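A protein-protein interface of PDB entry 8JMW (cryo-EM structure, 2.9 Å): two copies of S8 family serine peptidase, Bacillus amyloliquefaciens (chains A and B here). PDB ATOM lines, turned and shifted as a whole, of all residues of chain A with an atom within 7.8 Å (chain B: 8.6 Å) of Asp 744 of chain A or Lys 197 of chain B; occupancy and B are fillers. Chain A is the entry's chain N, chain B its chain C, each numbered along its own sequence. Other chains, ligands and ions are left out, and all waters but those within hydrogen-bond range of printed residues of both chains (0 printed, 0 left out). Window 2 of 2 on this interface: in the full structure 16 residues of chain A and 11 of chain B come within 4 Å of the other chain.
The side-chain hydroxyl of Tyr 739 of chain A lies close to the backbone carbonyl oxygen of Gln 202 of chain B (2.3 Å). The side-chain carboxylate of Asp 744 of chain A lies within salt-bridge range of the side-chain amino group of Lys 197 of chain B (3.98 Å).
The side-chain carboxylate (OD1) of Asp 740 of chain A lies within hydrogen-bond range of the backbone NH (N) of Leu 743 of chain A (2.8 Å). N of Tyr 739 of chain A sits at hydrogen-bond distance from O of Tyr 780 of chain A (2.9 Å). The backbone carbonyl oxygen of Gly 201 of chain B sits at hydrogen-bond distance from the side-chain amino group of Lys 204 of chain B (3.0 Å). The side-chain hydroxyl (OH) of Tyr 191 of chain B is in hydrogen-bond range of the side-chain carboxylate (OD2) of Asp 214 of chain B, 2.8 Å away. The side-chain carboxylate (OD1) of Asp 740 of chain A lies within hydrogen-bond range of the backbone NH (N) of Asp 744 of chain A (2.4 Å).
Leu 743 of chain A touches Gln 202 of chain B (CD2 to NE2, 3.1 Å). OH of Tyr 191 of chain B touches CD2 of Phe 745 of chain A, 3.8 Å away. Lys 204 of chain B touches Phe 745 of chain A. Phe 745 of chain A touches Asp 214 of chain B.
Printed residues of chain B within 4 Å of Leu 743 of chain A: Gln 202. Printed residues of chain B within 4 Å of Asp 744 of chain A: Lys 197. Of the printed residues of chain A, Tyr 191 of chain B touches Phe 745. Of the printed residues of chain A, Lys 197 of chain B touches Asp 744 (3.98 Å). Of the printed residues of chain A, Gln 202 of chain B touches Tyr 739 and Leu 743. Of the printed residues of chain A, Lys 204 of chain B touches Phe 745 (3.96 Å). Of the printed residues of chain A, Asp 214 of chain B touches Phe 745. Ala 239 of chain B touches none of the printed residues of chain A. The nearest printed residue of chain B that does not touch Asp 744 of chain A is Lys 204 of chain B (5.6 Å). The nearest printed residue of chain A that does not touch Lys 197 of chain B is Leu 743 of chain A (6.5 Å). The nearest printed residue of chain A that does not touch Asp 214 of chain B is Val 746 of chain A (5.5 Å).
Of the 23 printed residues of chain B, 5 touch a printed residue of chain A. Printed residues of chain B that touch a printed residue of chain A: Tyr 191, Lys 197, Gln 202, Lys 204 and Asp 214. Of the 12 printed residues of chain A, 4 touch a printed residue of chain B. Hydrophobic or aromatic side chains of chain A within 4 Å of the printed part of chain B: Tyr 739, Leu 743 and Phe 745. Among the printed residues, 6 pairs touch across the chains. Among the printed residues, Asp or Glu carboxylates within 4 Å of a Lys or Arg side-chain nitrogen of the other chain: Asp 744 of chain A with Lys 197 of chain B (3.98 Å).
No position is printed for both chains. Of the 6 pairs that touch across the chains among the printed residues, none has its exchanged pair printed and touching as well.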
ATOM      1  N   VAL A 738     -22.822  -7.590  26.519  1.00  0.00           N
ATOM      2  CA  VAL A 738     -24.249  -7.882  26.471  1.00  0.00           C
ATOM      3  C   VAL A 738     -24.459  -9.345  26.120  1.00  0.00           C
ATOM      4  O   VAL A 738     -23.804  -9.882  25.222  1.00  0.00           O
ATOM      5  CB  VAL A 738     -24.973  -6.976  25.462  1.00  0.00           C
ATOM      6  CG1 VAL A 738     -26.464  -7.114  25.623  1.00  0.00           C
ATOM      7  CG2 VAL A 738     -24.557  -5.545  25.663  1.00  0.00           C
ATOM      8  N   TYR A 739     -25.387  -9.985  26.824  1.00  0.00           N
ATOM      9  CA  TYR A 739     -25.734 -11.379  26.613  1.00  0.00           C
ATOM     10  C   TYR A 739     -27.229 -11.494  26.369  1.00  0.00           C
ATOM     11  O   TYR A 739     -28.020 -10.722  26.912  1.00  0.00           O
ATOM     12  CB  TYR A 739     -25.340 -12.228  27.817  1.00  0.00           C
ATOM     13  CG  TYR A 739     -23.856 -12.277  28.033  1.00  0.00           C
ATOM     14  CD1 TYR A 739     -23.081 -13.220  27.389  1.00  0.00           C
ATOM     15  CD2 TYR A 739     -23.232 -11.391  28.888  1.00  0.00           C
ATOM     16  CE1 TYR A 739     -21.727 -13.278  27.588  1.00  0.00           C
ATOM     17  CE2 TYR A 739     -21.878 -11.441  29.093  1.00  0.00           C
ATOM     18  CZ  TYR A 739     -21.132 -12.386  28.440  1.00  0.00           C
ATOM     19  OH  TYR A 739     -19.777 -12.443  28.641  1.00  0.00           O
ATOM     20  N   ASP A 740     -27.617 -12.462  25.547  1.00  0.00           N
ATOM     21  CA  ASP A 740     -29.028 -12.660  25.274  1.00  0.00           C
ATOM     22  C   ASP A 740     -29.687 -13.389  26.439  1.00  0.00           C
ATOM     23  O   ASP A 740     -29.060 -13.683  27.458  1.00  0.00           O
ATOM     24  CB  ASP A 740     -29.222 -13.412  23.961  1.00  0.00           C
ATOM     25  CG  ASP A 740     -28.612 -14.798  23.981  1.00  0.00           C
ATOM     26  OD1 ASP A 740     -28.047 -15.201  25.020  1.00  0.00           O
ATOM     27  OD2 ASP A 740     -28.702 -15.493  22.949  1.00  0.00           O
ATOM     28  N   SER A 741     -30.976 -13.689  26.287  1.00  0.00           N
ATOM     29  CA  SER A 741     -31.686 -14.415  27.332  1.00  0.00           C
ATOM     30  C   SER A 741     -31.114 -15.808  27.551  1.00  0.00           C
ATOM     31  O   SER A 741     -31.253 -16.358  28.647  1.00  0.00           O
ATOM     32  CB  SER A 741     -33.167 -14.516  26.989  1.00  0.00           C
ATOM     33  OG  SER A 741     -33.856 -15.260  27.977  1.00  0.00           O
ATOM     34  N   ASN A 742     -30.479 -16.386  26.537  1.00  0.00           N
ATOM     35  CA  ASN A 742     -29.836 -17.685  26.660  1.00  0.00           C
ATOM     36  C   ASN A 742     -28.394 -17.576  27.129  1.00  0.00           C
ATOM     37  O   ASN A 742     -27.657 -18.564  27.057  1.00  0.00           O
ATOM     38  CB  ASN A 742     -29.892 -18.426  25.326  1.00  0.00           C
ATOM     39  CG  ASN A 742     -31.284 -18.894  24.985  1.00  0.00           C
ATOM     40  OD1 ASN A 742     -31.788 -19.855  25.566  1.00  0.00           O
ATOM     41  ND2 ASN A 742     -31.921 -18.215  24.041  1.00  0.00           N
ATOM     42  N   LEU A 743     -27.982 -16.398  27.596  1.00  0.00           N
ATOM     43  CA  LEU A 743     -26.625 -16.167  28.081  1.00  0.00           C
ATOM     44  C   LEU A 743     -25.593 -16.457  26.996  1.00  0.00           C
ATOM     45  O   LEU A 743     -24.536 -17.032  27.253  1.00  0.00           O
ATOM     46  CB  LEU A 743     -26.342 -16.985  29.341  1.00  0.00           C
ATOM     47  CG  LEU A 743     -26.584 -16.280  30.675  1.00  0.00           C
ATOM     48  CD1 LEU A 743     -27.860 -15.471  30.645  1.00  0.00           C
ATOM     49  CD2 LEU A 743     -26.643 -17.301  31.790  1.00  0.00           C
ATOM     50  N   ASP A 744     -25.907 -16.057  25.770  1.00  0.00           N
ATOM     51  CA  ASP A 744     -24.980 -16.149  24.654  1.00  0.00           C
ATOM     52  C   ASP A 744     -24.398 -14.769  24.390  1.00  0.00           C
ATOM     53  O   ASP A 744     -25.137 -13.783  24.327  1.00  0.00           O
ATOM     54  CB  ASP A 744     -25.678 -16.678  23.404  1.00  0.00           C
ATOM     55  CG  ASP A 744     -26.134 -18.109  23.563  1.00  0.00           C
ATOM     56  OD1 ASP A 744     -25.701 -18.765  24.533  1.00  0.00           O
ATOM     57  OD2 ASP A 744     -26.927 -18.577  22.722  1.00  0.00           O
ATOM     58  N   PHE A 745     -23.080 -14.704  24.234  1.00  0.00           N
ATOM     59  CA  PHE A 745     -22.411 -13.419  24.095  1.00  0.00           C
ATOM     60  C   PHE A 745     -22.852 -12.714  22.824  1.00  0.00           C
ATOM     61  O   PHE A 745     -22.461 -13.105  21.721  1.00  0.00           O
ATOM     62  CB  PHE A 745     -20.894 -13.603  24.107  1.00  0.00           C
ATOM     63  CG  PHE A 745     -20.136 -12.334  23.886  1.00  0.00           C
ATOM     64  CD1 PHE A 745     -19.923 -11.456  24.925  1.00  0.00           C
ATOM     65  CD2 PHE A 745     -19.623 -12.026  22.644  1.00  0.00           C
ATOM     66  CE1 PHE A 745     -19.228 -10.290  24.726  1.00  0.00           C
ATOM     67  CE2 PHE A 745     -18.927 -10.861  22.442  1.00  0.00           C
ATOM     68  CZ  PHE A 745     -18.729  -9.992  23.486  1.00  0.00           C
ATOM     69  N   VAL A 746     -23.667 -11.674  22.972  1.00  0.00           N
ATOM     70  CA  VAL A 746     -24.122 -10.926  21.809  1.00  0.00           C
ATOM     71  C   VAL A 746     -23.037  -9.986  21.315  1.00  0.00           C
ATOM     72  O   VAL A 746     -22.748  -9.932  20.118  1.00  0.00           O
ATOM     73  CB  VAL A 746     -25.415 -10.167  22.140  1.00  0.00           C
ATOM     74  CG1 VAL A 746     -25.795  -9.277  20.984  1.00  0.00           C
ATOM     75  CG2 VAL A 746     -26.529 -11.143  22.448  1.00  0.00           C
ATOM     76  N   GLY A 747     -22.417  -9.237  22.218  1.00  0.00           N
ATOM     77  CA  GLY A 747     -21.367  -8.327  21.810  1.00  0.00           C
ATOM     78  C   GLY A 747     -20.916  -7.457  22.964  1.00  0.00           C
ATOM     79  O   GLY A 747     -21.144  -7.779  24.129  1.00  0.00           O
ATOM     80  N   TYR A 779     -32.202  -9.058  27.809  1.00  0.00           N
ATOM     81  CA  TYR A 779     -30.750  -9.107  27.781  1.00  0.00           C
ATOM     82  C   TYR A 779     -30.179  -8.970  29.182  1.00  0.00           C
ATOM     83  O   TYR A 779     -30.790  -8.384  30.077  1.00  0.00           O
ATOM     84  CB  TYR A 779     -30.178  -8.007  26.890  1.00  0.00           C
ATOM     85  CG  TYR A 779     -30.438  -8.235  25.431  1.00  0.00           C
ATOM     86  CD1 TYR A 779     -30.171  -9.456  24.849  1.00  0.00           C
ATOM     87  CD2 TYR A 779     -30.957  -7.232  24.637  1.00  0.00           C
ATOM     88  CE1 TYR A 779     -30.406  -9.674  23.516  1.00  0.00           C
ATOM     89  CE2 TYR A 779     -31.198  -7.439  23.303  1.00  0.00           C
ATOM     90  CZ  TYR A 779     -30.921  -8.663  22.748  1.00  0.00           C
ATOM     91  OH  TYR A 779     -31.157  -8.879  21.415  1.00  0.00           O
ATOM     92  N   TYR A 780     -28.975  -9.506  29.344  1.00  0.00           N
ATOM     93  CA  TYR A 780     -28.176  -9.363  30.548  1.00  0.00           C
ATOM     94  C   TYR A 780     -26.937  -8.561  30.198  1.00  0.00           C
ATOM     95  O   TYR A 780     -26.504  -8.546  29.046  1.00  0.00           O
ATOM     96  CB  TYR A 780     -27.748 -10.710  31.100  1.00  0.00           C
ATOM     97  CG  TYR A 780     -28.876 -11.565  31.593  1.00  0.00           C
ATOM     98  CD1 TYR A 780     -29.572 -12.383  30.724  1.00  0.00           C
ATOM     99  CD2 TYR A 780     -29.230 -11.576  32.927  1.00  0.00           C
ATOM    100  CE1 TYR A 780     -30.597 -13.174  31.165  1.00  0.00           C
ATOM    101  CE2 TYR A 780     -30.254 -12.365  33.380  1.00  0.00           C
ATOM    102  CZ  TYR A 780     -30.935 -13.164  32.494  1.00  0.00           C
ATOM    103  OH  TYR A 780     -31.964 -13.957  32.938  1.00  0.00           O
ATOM    104  N   VAL B 189     -10.453 -19.172  20.243  1.00  0.00           N
ATOM    105  CA  VAL B 189     -11.258 -20.369  20.432  1.00  0.00           C
ATOM    106  C   VAL B 189     -12.667 -20.096  19.938  1.00  0.00           C
ATOM    107  O   VAL B 189     -13.251 -19.056  20.257  1.00  0.00           O
ATOM    108  CB  VAL B 189     -11.288 -20.811  21.906  1.00  0.00           C
ATOM    109  CG1 VAL B 189     -12.154 -22.033  22.069  1.00  0.00           C
ATOM    110  CG2 VAL B 189      -9.890 -21.085  22.399  1.00  0.00           C
ATOM    111  N   GLU B 190     -13.208 -21.023  19.156  1.00  0.00           N
ATOM    112  CA  GLU B 190     -14.608 -20.969  18.745  1.00  0.00           C
ATOM    113  C   GLU B 190     -15.445 -21.441  19.926  1.00  0.00           C
ATOM    114  O   GLU B 190     -15.718 -22.628  20.091  1.00  0.00           O
ATOM    115  CB  GLU B 190     -14.834 -21.820  17.504  1.00  0.00           C
ATOM    116  CG  GLU B 190     -16.286 -22.078  17.156  1.00  0.00           C
ATOM    117  CD  GLU B 190     -17.073 -20.807  16.941  1.00  0.00           C
ATOM    118  OE1 GLU B 190     -17.613 -20.268  17.929  1.00  0.00           O
ATOM    119  OE2 GLU B 190     -17.158 -20.348  15.783  1.00  0.00           O
ATOM    120  N   TYR B 191     -15.852 -20.499  20.777  1.00  0.00           N
ATOM    121  CA  TYR B 191     -16.614 -20.849  21.973  1.00  0.00           C
ATOM    122  C   TYR B 191     -18.095 -21.025  21.689  1.00  0.00           C
ATOM    123  O   TYR B 191     -18.945 -20.563  22.451  1.00  0.00           O
ATOM    124  CB  TYR B 191     -16.400 -19.772  23.031  1.00  0.00           C
ATOM    125  CG  TYR B 191     -16.633 -18.377  22.511  1.00  0.00           C
ATOM    126  CD1 TYR B 191     -17.907 -17.844  22.446  1.00  0.00           C
ATOM    127  CD2 TYR B 191     -15.577 -17.595  22.086  1.00  0.00           C
ATOM    128  CE1 TYR B 191     -18.126 -16.583  21.967  1.00  0.00           C
ATOM    129  CE2 TYR B 191     -15.787 -16.326  21.611  1.00  0.00           C
ATOM    130  CZ  TYR B 191     -17.064 -15.827  21.551  1.00  0.00           C
ATOM    131  OH  TYR B 191     -17.284 -14.561  21.077  1.00  0.00           O
ATOM    132  N   LYS B 192     -18.421 -21.744  20.629  1.00  0.00           N
ATOM    133  CA  LYS B 192     -19.796 -22.095  20.329  1.00  0.00           C
ATOM    134  C   LYS B 192     -19.902 -23.533  19.871  1.00  0.00           C
ATOM    135  O   LYS B 192     -21.012 -24.004  19.607  1.00  0.00           O
ATOM    136  CB  LYS B 192     -20.376 -21.168  19.256  1.00  0.00           C
ATOM    137  CG  LYS B 192     -20.553 -19.736  19.699  1.00  0.00           C
ATOM    138  CD  LYS B 192     -21.103 -18.896  18.570  1.00  0.00           C
ATOM    139  CE  LYS B 192     -21.312 -17.461  19.002  1.00  0.00           C
ATOM    140  NZ  LYS B 192     -21.824 -16.630  17.882  1.00  0.00           N
ATOM    141  N   HIS B 193     -18.784 -24.229  19.755  1.00  0.00           N
ATOM    142  CA  HIS B 193     -18.807 -25.653  19.509  1.00  0.00           C
ATOM    143  C   HIS B 193     -19.601 -26.325  20.619  1.00  0.00           C
ATOM    144  O   HIS B 193     -19.369 -26.034  21.799  1.00  0.00           O
ATOM    145  CB  HIS B 193     -17.379 -26.185  19.471  1.00  0.00           C
ATOM    146  CG  HIS B 193     -17.222 -27.450  18.695  1.00  0.00           C
ATOM    147  ND1 HIS B 193     -17.839 -28.626  19.056  1.00  0.00           N
ATOM    148  CD2 HIS B 193     -16.507 -27.726  17.581  1.00  0.00           C
ATOM    149  CE1 HIS B 193     -17.515 -29.572  18.195  1.00  0.00           C
ATOM    150  NE2 HIS B 193     -16.707 -29.052  17.291  1.00  0.00           N
ATOM    151  N   PRO B 194     -20.551 -27.201  20.294  1.00  0.00           N
ATOM    152  CA  PRO B 194     -21.372 -27.811  21.350  1.00  0.00           C
ATOM    153  C   PRO B 194     -20.557 -28.531  22.399  1.00  0.00           C
ATOM    154  O   PRO B 194     -21.005 -28.632  23.548  1.00  0.00           O
ATOM    155  CB  PRO B 194     -22.272 -28.780  20.577  1.00  0.00           C
ATOM    156  CG  PRO B 194     -22.311 -28.240  19.197  1.00  0.00           C
ATOM    157  CD  PRO B 194     -20.987 -27.597  18.949  1.00  0.00           C
ATOM    158  N   ASP B 195     -19.373 -29.027  22.050  1.00  0.00           N
ATOM    159  CA  ASP B 195     -18.504 -29.670  23.021  1.00  0.00           C
ATOM    160  C   ASP B 195     -17.794 -28.678  23.928  1.00  0.00           C
ATOM    161  O   ASP B 195     -17.320 -29.071  24.997  1.00  0.00           O
ATOM    162  CB  ASP B 195     -17.475 -30.533  22.298  1.00  0.00           C
ATOM    163  CG  ASP B 195     -18.052 -31.845  21.828  1.00  0.00           C
ATOM    164  OD1 ASP B 195     -19.210 -32.146  22.183  1.00  0.00           O
ATOM    165  OD2 ASP B 195     -17.351 -32.577  21.101  1.00  0.00           O
ATOM    166  N   LEU B 196     -17.716 -27.408  23.537  1.00  0.00           N
ATOM    167  CA  LEU B 196     -17.040 -26.389  24.322  1.00  0.00           C
ATOM    168  C   LEU B 196     -17.985 -25.363  24.917  1.00  0.00           C
ATOM    169  O   LEU B 196     -17.533 -24.498  25.672  1.00  0.00           O
ATOM    170  CB  LEU B 196     -16.006 -25.655  23.460  1.00  0.00           C
ATOM    171  CG  LEU B 196     -14.876 -26.475  22.856  1.00  0.00           C
ATOM    172  CD1 LEU B 196     -13.964 -25.572  22.064  1.00  0.00           C
ATOM    173  CD2 LEU B 196     -14.107 -27.175  23.946  1.00  0.00           C
ATOM    174  N   LYS B 197     -19.277 -25.431  24.600  1.00  0.00           N
ATOM    175  CA  LYS B 197     -20.189 -24.356  24.965  1.00  0.00           C
ATOM    176  C   LYS B 197     -20.299 -24.200  26.475  1.00  0.00           C
ATOM    177  O   LYS B 197     -20.243 -23.080  26.993  1.00  0.00           O
ATOM    178  CB  LYS B 197     -21.563 -24.618  24.357  1.00  0.00           C
ATOM    179  CG  LYS B 197     -22.180 -23.415  23.690  1.00  0.00           C
ATOM    180  CD  LYS B 197     -23.504 -23.770  23.051  1.00  0.00           C
ATOM    181  CE  LYS B 197     -23.906 -22.730  22.025  1.00  0.00           C
ATOM    182  NZ  LYS B 197     -23.510 -21.362  22.455  1.00  0.00           N
ATOM    183  N   LYS B 198     -20.452 -25.304  27.198  1.00  0.00           N
ATOM    184  CA  LYS B 198     -20.715 -25.228  28.626  1.00  0.00           C
ATOM    185  C   LYS B 198     -19.458 -25.082  29.465  1.00  0.00           C
ATOM    186  O   LYS B 198     -19.561 -24.795  30.659  1.00  0.00           O
ATOM    187  CB  LYS B 198     -21.487 -26.464  29.087  1.00  0.00           C
ATOM    188  CG  LYS B 198     -21.249 -27.697  28.248  1.00  0.00           C
ATOM    189  CD  LYS B 198     -21.696 -28.942  28.993  1.00  0.00           C
ATOM    190  CE  LYS B 198     -21.761 -30.146  28.072  1.00  0.00           C
ATOM    191  NZ  LYS B 198     -21.604 -31.419  28.823  1.00  0.00           N
ATOM    192  N   ASN B 199     -18.279 -25.266  28.879  1.00  0.00           N
ATOM    193  CA  ASN B 199     -17.042 -25.064  29.613  1.00  0.00           C
ATOM    194  C   ASN B 199     -16.617 -23.608  29.654  1.00  0.00           C
ATOM    195  O   ASN B 199     -15.754 -23.252  30.462  1.00  0.00           O
ATOM    196  CB  ASN B 199     -15.923 -25.906  29.005  1.00  0.00           C
ATOM    197  CG  ASN B 199     -15.912 -27.317  29.536  1.00  0.00           C
ATOM    198  OD1 ASN B 199     -16.760 -27.693  30.341  1.00  0.00           O
ATOM    199  ND2 ASN B 199     -14.955 -28.112  29.082  1.00  0.00           N
ATOM    200  N   PHE B 200     -17.193 -22.765  28.809  1.00  0.00           N
ATOM    201  CA  PHE B 200     -16.882 -21.346  28.826  1.00  0.00           C
ATOM    202  C   PHE B 200     -17.834 -20.616  29.758  1.00  0.00           C
ATOM    203  O   PHE B 200     -19.049 -20.823  29.707  1.00  0.00           O
ATOM    204  CB  PHE B 200     -16.969 -20.767  27.420  1.00  0.00           C
ATOM    205  CG  PHE B 200     -15.703 -20.897  26.649  1.00  0.00           C
ATOM    206  CD1 PHE B 200     -14.723 -19.936  26.747  1.00  0.00           C
ATOM    207  CD2 PHE B 200     -15.483 -21.988  25.840  1.00  0.00           C
ATOM    208  CE1 PHE B 200     -13.555 -20.055  26.046  1.00  0.00           C
ATOM    209  CE2 PHE B 200     -14.315 -22.111  25.138  1.00  0.00           C
ATOM    210  CZ  PHE B 200     -13.351 -21.144  25.242  1.00  0.00           C
ATOM    211  N   GLY B 201     -17.282 -19.761  30.606  1.00  0.00           N
ATOM    212  CA  GLY B 201     -18.103 -18.983  31.509  1.00  0.00           C
ATOM    213  C   GLY B 201     -18.761 -17.823  30.803  1.00  0.00           C
ATOM    214  O   GLY B 201     -18.889 -17.826  29.577  1.00  0.00           O
ATOM    215  N   GLN B 202     -19.196 -16.822  31.564  1.00  0.00           N
ATOM    216  CA  GLN B 202     -19.819 -15.657  30.951  1.00  0.00           C
ATOM    217  C   GLN B 202     -18.777 -14.879  30.165  1.00  0.00           C
ATOM    218  O   GLN B 202     -18.961 -14.591  28.978  1.00  0.00           O
ATOM    219  CB  GLN B 202     -20.494 -14.806  32.024  1.00  0.00           C
ATOM    220  CG  GLN B 202     -21.734 -15.441  32.604  1.00  0.00           C
ATOM    221  CD  GLN B 202     -22.768 -15.779  31.556  1.00  0.00           C
ATOM    222  OE1 GLN B 202     -22.773 -15.220  30.461  1.00  0.00           O
ATOM    223  NE2 GLN B 202     -23.635 -16.723  31.878  1.00  0.00           N
ATOM    224  N   LYS B 204     -15.608 -14.740  28.142  1.00  0.00           N
ATOM    225  CA  LYS B 204     -14.908 -15.750  27.362  1.00  0.00           C
ATOM    226  C   LYS B 204     -13.416 -15.497  27.251  1.00  0.00           C
ATOM    227  O   LYS B 204     -12.646 -16.451  27.108  1.00  0.00           O
ATOM    228  CB  LYS B 204     -15.514 -15.842  25.964  1.00  0.00           C
ATOM    229  CG  LYS B 204     -16.999 -15.594  25.946  1.00  0.00           C
ATOM    230  CD  LYS B 204     -17.744 -16.892  26.135  1.00  0.00           C
ATOM    231  CE  LYS B 204     -19.222 -16.721  25.887  1.00  0.00           C
ATOM    232  NZ  LYS B 204     -20.015 -17.595  26.785  1.00  0.00           N
ATOM    233  N   ASP B 214     -14.278 -10.547  21.924  1.00  0.00           N
ATOM    234  CA  ASP B 214     -14.783 -11.663  21.131  1.00  0.00           C
ATOM    235  C   ASP B 214     -13.587 -12.434  20.594  1.00  0.00           C
ATOM    236  O   ASP B 214     -13.105 -12.158  19.483  1.00  0.00           O
ATOM    237  CB  ASP B 214     -15.669 -11.162  19.995  1.00  0.00           C
ATOM    238  CG  ASP B 214     -16.559 -12.241  19.436  1.00  0.00           C
ATOM    239  OD1 ASP B 214     -16.037 -13.145  18.753  1.00  0.00           O
ATOM    240  OD2 ASP B 214     -17.781 -12.193  19.682  1.00  0.00           O
ATOM    241  N   ALA B 239     -10.305 -29.408  27.547  1.00  0.00           N
ATOM    242  CA  ALA B 239     -11.553 -29.599  28.277  1.00  0.00           C
ATOM    243  C   ALA B 239     -12.707 -29.488  27.289  1.00  0.00           C
ATOM    244  O   ALA B 239     -13.203 -28.388  27.035  1.00  0.00           O
ATOM    245  CB  ALA B 239     -11.685 -28.577  29.394  1.00  0.00           C
ATOM    246  N   ALA B 240     -13.133 -30.624  26.752  1.00  0.00           N
ATOM    247  CA  ALA B 240     -14.302 -30.694  25.889  1.00  0.00           C
ATOM    248  C   ALA B 240     -15.250 -31.717  26.484  1.00  0.00           C
ATOM    249  O   ALA B 240     -14.843 -32.845  26.766  1.00  0.00           O
ATOM    250  CB  ALA B 240     -13.923 -31.080  24.460  1.00  0.00           C
ATOM    251  N   ASN B 241     -16.497 -31.321  26.694  1.00  0.00           N
ATOM    252  CA  ASN B 241     -17.508 -32.202  27.259  1.00  0.00           C
ATOM    253  C   ASN B 241     -18.565 -32.474  26.200  1.00  0.00           C
ATOM    254  O   ASN B 241     -19.181 -31.539  25.680  1.00  0.00           O
ATOM    255  CB  ASN B 241     -18.138 -31.585  28.503  1.00  0.00           C
ATOM    256  CG  ASN B 241     -18.333 -32.593  29.605  1.00  0.00           C
ATOM    257  OD1 ASN B 241     -18.378 -33.795  29.357  1.00  0.00           O
ATOM    258  ND2 ASN B 241     -18.445 -32.109  30.834  1.00  0.00           N
ATOM    259  N   GLY B 242     -18.772 -33.746  25.886  1.00  0.00           N
ATOM    260  CA  GLY B 242     -19.750 -34.114  24.885  1.00  0.00           C
ATOM    261  C   GLY B 242     -19.338 -35.334  24.092  1.00  0.00           C
ATOM    262  O   GLY B 242     -18.969 -36.361  24.667  1.00  0.00           O
ATOM    263  N   LEU B 253     -12.851 -22.344  30.864  1.00  0.00           N
ATOM    264  CA  LEU B 253     -11.910 -21.987  29.819  1.00  0.00           C
ATOM    265  C   LEU B 253     -11.931 -20.488  29.586  1.00  0.00           C
ATOM    266  O   LEU B 253     -12.976 -19.847  29.708  1.00  0.00           O
ATOM    267  CB  LEU B 253     -12.234 -22.708  28.516  1.00  0.00           C
ATOM    268  CG  LEU B 253     -11.775 -24.156  28.416  1.00  0.00           C
ATOM    269  CD1 LEU B 253     -12.628 -24.897  27.418  1.00  0.00           C
ATOM    270  CD2 LEU B 253     -10.322 -24.217  28.022  1.00  0.00           C
ATOM    271  N   THR B 512     -12.034 -30.916  18.620  1.00  0.00           N
ATOM    272  CA  THR B 512     -13.017 -30.006  18.056  1.00  0.00           C
ATOM    273  C   THR B 512     -12.344 -28.943  17.205  1.00  0.00           C
ATOM    274  O   THR B 512     -11.350 -28.345  17.616  1.00  0.00           O
ATOM    275  CB  THR B 512     -13.802 -29.346  19.180  1.00  0.00           C
ATOM    276  OG1 THR B 512     -12.889 -28.675  20.054  1.00  0.00           O
ATOM    277  CG2 THR B 512     -14.543 -30.388  19.977  1.00  0.00           C
ATOM    278  N   TYR B 522     -19.152 -26.350  13.065  1.00  0.00           N
ATOM    279  CA  TYR B 522     -18.409 -27.109  14.059  1.00  0.00           C
ATOM    280  C   TYR B 522     -18.200 -28.538  13.589  1.00  0.00           C
ATOM    281  O   TYR B 522     -19.103 -29.151  13.015  1.00  0.00           O
ATOM    282  CB  TYR B 522     -19.140 -27.099  15.398  1.00  0.00           C
ATOM    283  CG  TYR B 522     -19.794 -25.778  15.695  1.00  0.00           C
ATOM    284  CD1 TYR B 522     -19.057 -24.605  15.692  1.00  0.00           C
ATOM    285  CD2 TYR B 522     -21.149 -25.697  15.959  1.00  0.00           C
ATOM    286  CE1 TYR B 522     -19.648 -23.392  15.954  1.00  0.00           C
ATOM    287  CE2 TYR B 522     -21.751 -24.489  16.222  1.00  0.00           C
ATOM    288  CZ  TYR B 522     -20.996 -23.341  16.218  1.00  0.00           C
ATOM    289  OH  TYR B 522     -21.594 -22.132  16.481  1.00  0.00           O
